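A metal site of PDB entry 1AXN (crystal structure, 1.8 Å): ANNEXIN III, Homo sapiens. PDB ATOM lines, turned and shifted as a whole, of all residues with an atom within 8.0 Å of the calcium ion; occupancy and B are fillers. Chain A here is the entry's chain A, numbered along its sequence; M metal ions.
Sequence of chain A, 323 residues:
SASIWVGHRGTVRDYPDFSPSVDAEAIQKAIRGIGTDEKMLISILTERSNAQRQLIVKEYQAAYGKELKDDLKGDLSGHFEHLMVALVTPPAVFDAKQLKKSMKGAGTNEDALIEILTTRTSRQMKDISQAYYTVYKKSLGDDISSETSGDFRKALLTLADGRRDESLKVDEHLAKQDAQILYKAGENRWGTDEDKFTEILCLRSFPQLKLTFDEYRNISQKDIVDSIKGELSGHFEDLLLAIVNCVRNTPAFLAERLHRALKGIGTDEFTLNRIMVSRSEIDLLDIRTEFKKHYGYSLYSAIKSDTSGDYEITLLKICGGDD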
ATOM      1  N   GLN A  28      19.181  21.244  -5.682  1.00  0.00           N
ATOM      2  CA  GLN A  28      17.814  21.765  -5.755  1.00  0.00           C
ATOM      3  C   GLN A  28      17.465  22.597  -4.534  1.00  0.00           C
ATOM      4  O   GLN A  28      16.953  23.701  -4.688  1.00  0.00           O
ATOM      5  CB  GLN A  28      16.843  20.622  -5.960  1.00  0.00           C
ATOM      6  CG  GLN A  28      15.426  20.914  -5.443  1.00  0.00           C
ATOM      7  CD  GLN A  28      14.662  21.704  -6.467  1.00  0.00           C
ATOM      8  OE1 GLN A  28      13.484  21.994  -6.278  1.00  0.00           O
ATOM      9  NE2 GLN A  28      15.329  22.054  -7.562  1.00  0.00           N
ATOM     10  N   LYS A  29      17.735  22.112  -3.337  1.00  0.00           N
ATOM     11  CA  LYS A  29      17.412  22.868  -2.139  1.00  0.00           C
ATOM     12  C   LYS A  29      18.164  24.196  -2.157  1.00  0.00           C
ATOM     13  O   LYS A  29      17.661  25.251  -1.748  1.00  0.00           O
ATOM     14  CB  LYS A  29      17.670  22.030  -0.896  1.00  0.00           C
ATOM     15  CG  LYS A  29      18.770  22.344   0.057  1.00  0.00           C
ATOM     16  CD  LYS A  29      20.087  21.630  -0.194  1.00  0.00           C
ATOM     17  CE  LYS A  29      21.269  22.533   0.118  1.00  0.00           C
ATOM     18  NZ  LYS A  29      22.596  22.030  -0.255  1.00  0.00           N
ATOM     19  N   ALA A  30      19.402  24.187  -2.634  1.00  0.00           N
ATOM     20  CA  ALA A  30      20.275  25.338  -2.713  1.00  0.00           C
ATOM     21  C   ALA A  30      19.786  26.463  -3.609  1.00  0.00           C
ATOM     22  O   ALA A  30      20.112  27.619  -3.299  1.00  0.00           O
ATOM     23  CB  ALA A  30      21.679  24.881  -3.110  1.00  0.00           C
ATOM     24  N   ILE A  31      19.051  26.192  -4.677  1.00  0.00           N
ATOM     25  CA  ILE A  31      18.623  27.311  -5.520  1.00  0.00           C
ATOM     26  C   ILE A  31      17.149  27.600  -5.345  1.00  0.00           C
ATOM     27  O   ILE A  31      16.636  28.675  -5.641  1.00  0.00           O
ATOM     28  CB  ILE A  31      18.980  27.070  -7.007  1.00  0.00           C
ATOM     29  CG1 ILE A  31      18.100  25.987  -7.613  1.00  0.00           C
ATOM     30  CG2 ILE A  31      20.448  26.733  -7.177  1.00  0.00           C
ATOM     31  CD1 ILE A  31      18.492  25.549  -8.992  1.00  0.00           C
ATOM     32  N   ARG A  32      16.430  26.599  -4.852  1.00  0.00           N
ATOM     33  CA  ARG A  32      14.999  26.704  -4.638  1.00  0.00           C
ATOM     34  C   ARG A  32      14.613  27.893  -3.771  1.00  0.00           C
ATOM     35  O   ARG A  32      15.205  28.161  -2.715  1.00  0.00           O
ATOM     36  CB  ARG A  32      14.584  25.391  -3.981  1.00  0.00           C
ATOM     37  CG  ARG A  32      13.182  24.908  -4.291  1.00  0.00           C
ATOM     38  CD  ARG A  32      12.557  24.670  -2.941  1.00  0.00           C
ATOM     39  NE  ARG A  32      12.390  23.374  -2.381  1.00  0.00           N
ATOM     40  CZ  ARG A  32      12.147  22.177  -2.853  1.00  0.00           C
ATOM     41  NH1 ARG A  32      12.044  21.921  -4.150  1.00  0.00           N
ATOM     42  NH2 ARG A  32      12.026  21.175  -1.992  1.00  0.00           N
ATOM     43  N   GLY A  33      13.601  28.642  -4.212  1.00  0.00           N
ATOM     44  CA  GLY A  33      13.123  29.794  -3.475  1.00  0.00           C
ATOM     45  C   GLY A  33      13.877  31.093  -3.589  1.00  0.00           C
ATOM     46  O   GLY A  33      14.577  31.333  -4.571  1.00  0.00           O
ATOM     47  N   ILE A  34      13.738  31.957  -2.574  1.00  0.00           N
ATOM     48  CA  ILE A  34      14.427  33.241  -2.632  1.00  0.00           C
ATOM     49  C   ILE A  34      15.876  33.008  -2.217  1.00  0.00           C
ATOM     50  O   ILE A  34      16.161  32.292  -1.272  1.00  0.00           O
ATOM     51  CB  ILE A  34      13.843  34.387  -1.782  1.00  0.00           C
ATOM     52  CG1 ILE A  34      12.600  35.038  -2.404  1.00  0.00           C
ATOM     53  CG2 ILE A  34      14.863  35.515  -1.534  1.00  0.00           C
ATOM     54  CD1 ILE A  34      12.028  36.169  -1.565  1.00  0.00           C
ATOM     55  N   GLY A  35      16.755  33.652  -2.963  1.00  0.00           N
ATOM     56  CA  GLY A  35      18.169  33.537  -2.656  1.00  0.00           C
ATOM     57  C   GLY A  35      18.698  32.249  -3.288  1.00  0.00           C
ATOM     58  O   GLY A  35      18.013  31.493  -3.971  1.00  0.00           O
ATOM     59  N   THR A  36      19.974  32.090  -2.977  1.00  0.00           N
ATOM     60  CA  THR A  36      20.702  30.949  -3.486  1.00  0.00           C
ATOM     61  C   THR A  36      21.814  30.596  -2.533  1.00  0.00           C
ATOM     62  O   THR A  36      22.442  31.516  -1.987  1.00  0.00           O
ATOM     63  CB  THR A  36      21.321  31.381  -4.842  1.00  0.00           C
ATOM     64  OG1 THR A  36      20.236  31.872  -5.638  1.00  0.00           O
ATOM     65  CG2 THR A  36      22.043  30.222  -5.497  1.00  0.00           C
ATOM     66  N   ASP A  37      22.026  29.302  -2.336  1.00  0.00           N
ATOM     67  CA  ASP A  37      23.136  28.927  -1.450  1.00  0.00           C
ATOM     68  C   ASP A  37      24.304  28.715  -2.436  1.00  0.00           C
ATOM     69  O   ASP A  37      24.567  27.581  -2.825  1.00  0.00           O
ATOM     70  CB  ASP A  37      22.835  27.720  -0.593  1.00  0.00           C
ATOM     71  CG  ASP A  37      23.896  27.415   0.451  1.00  0.00           C
ATOM     72  OD1 ASP A  37      24.962  28.060   0.485  1.00  0.00           O
ATOM     73  OD2 ASP A  37      23.662  26.512   1.287  1.00  0.00           O
ATOM     74  N   ASP A  71      18.371  26.118 -14.468  1.00  0.00           N
ATOM     75  CA  ASP A  71      18.162  26.642 -13.117  1.00  0.00           C
ATOM     76  C   ASP A  71      19.357  27.486 -12.707  1.00  0.00           C
ATOM     77  O   ASP A  71      19.232  28.508 -12.039  1.00  0.00           O
ATOM     78  CB  ASP A  71      17.931  25.521 -12.121  1.00  0.00           C
ATOM     79  CG  ASP A  71      16.469  25.125 -12.108  1.00  0.00           C
ATOM     80  OD1 ASP A  71      15.680  25.732 -12.850  1.00  0.00           O
ATOM     81  OD2 ASP A  71      16.127  24.198 -11.367  1.00  0.00           O
ATOM     82  N   GLY A  74      19.096  30.864 -14.287  1.00  0.00           N
ATOM     83  CA  GLY A  74      18.046  31.678 -13.693  1.00  0.00           C
ATOM     84  C   GLY A  74      18.393  32.268 -12.338  1.00  0.00           C
ATOM     85  O   GLY A  74      17.917  33.336 -11.970  1.00  0.00           O
ATOM     86  N   ASP A  75      19.244  31.580 -11.577  1.00  0.00           N
ATOM     87  CA  ASP A  75      19.648  32.015 -10.258  1.00  0.00           C
ATOM     88  C   ASP A  75      20.974  32.718 -10.133  1.00  0.00           C
ATOM     89  O   ASP A  75      21.097  33.573  -9.270  1.00  0.00           O
ATOM     90  CB  ASP A  75      19.839  30.757  -9.364  1.00  0.00           C
ATOM     91  CG  ASP A  75      18.736  30.563  -8.342  1.00  0.00           C
ATOM     92  OD1 ASP A  75      17.547  30.604  -8.731  1.00  0.00           O
ATOM     93  OD2 ASP A  75      19.063  30.360  -7.148  1.00  0.00           O
ATOM     94  N   LEU A  76      21.917  32.303 -10.984  1.00  0.00           N
ATOM     95  CA  LEU A  76      23.235  32.898 -10.917  1.00  0.00           C
ATOM     96  C   LEU A  76      23.433  34.029 -11.940  1.00  0.00           C
ATOM     97  O   LEU A  76      22.704  34.059 -12.909  1.00  0.00           O
ATOM     98  CB  LEU A  76      24.291  31.810 -11.107  1.00  0.00           C
ATOM     99  CG  LEU A  76      24.185  30.574 -10.206  1.00  0.00           C
ATOM    100  CD1 LEU A  76      25.449  29.729 -10.328  1.00  0.00           C
ATOM    101  CD2 LEU A  76      23.948  30.970  -8.747  1.00  0.00           C
HETATM  102 CA    CA M   1      16.827  30.948  -5.735  1.00  0.00          CA
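OG1 of Thr 36 lies close to OD2 of Asp 75 (2.4 Å).
Residues that only touch the calcium ion: Thr 36. Five residues have an atom within 4 Å of the calcium ion: Ile 31, Gly 33, Gly 35, Thr 36 and Asp 75.
The backbone carbonyl oxygen (O) of Gly 35 is bound to the calcium ion, 2.2 Å away. The calcium ion is bound by O of Ile 31 (2.3 Å). O of Gly 33 binds the calcium ion (2.6 Å). OD2 of Asp 75 is bound to the calcium ion (2.7 Å). The calcium ion has four donor atoms within binding distance. Slightly farther from the calcium ion lies the side-chain carboxylate (OD1) of Asp 75 (3.1 Å).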
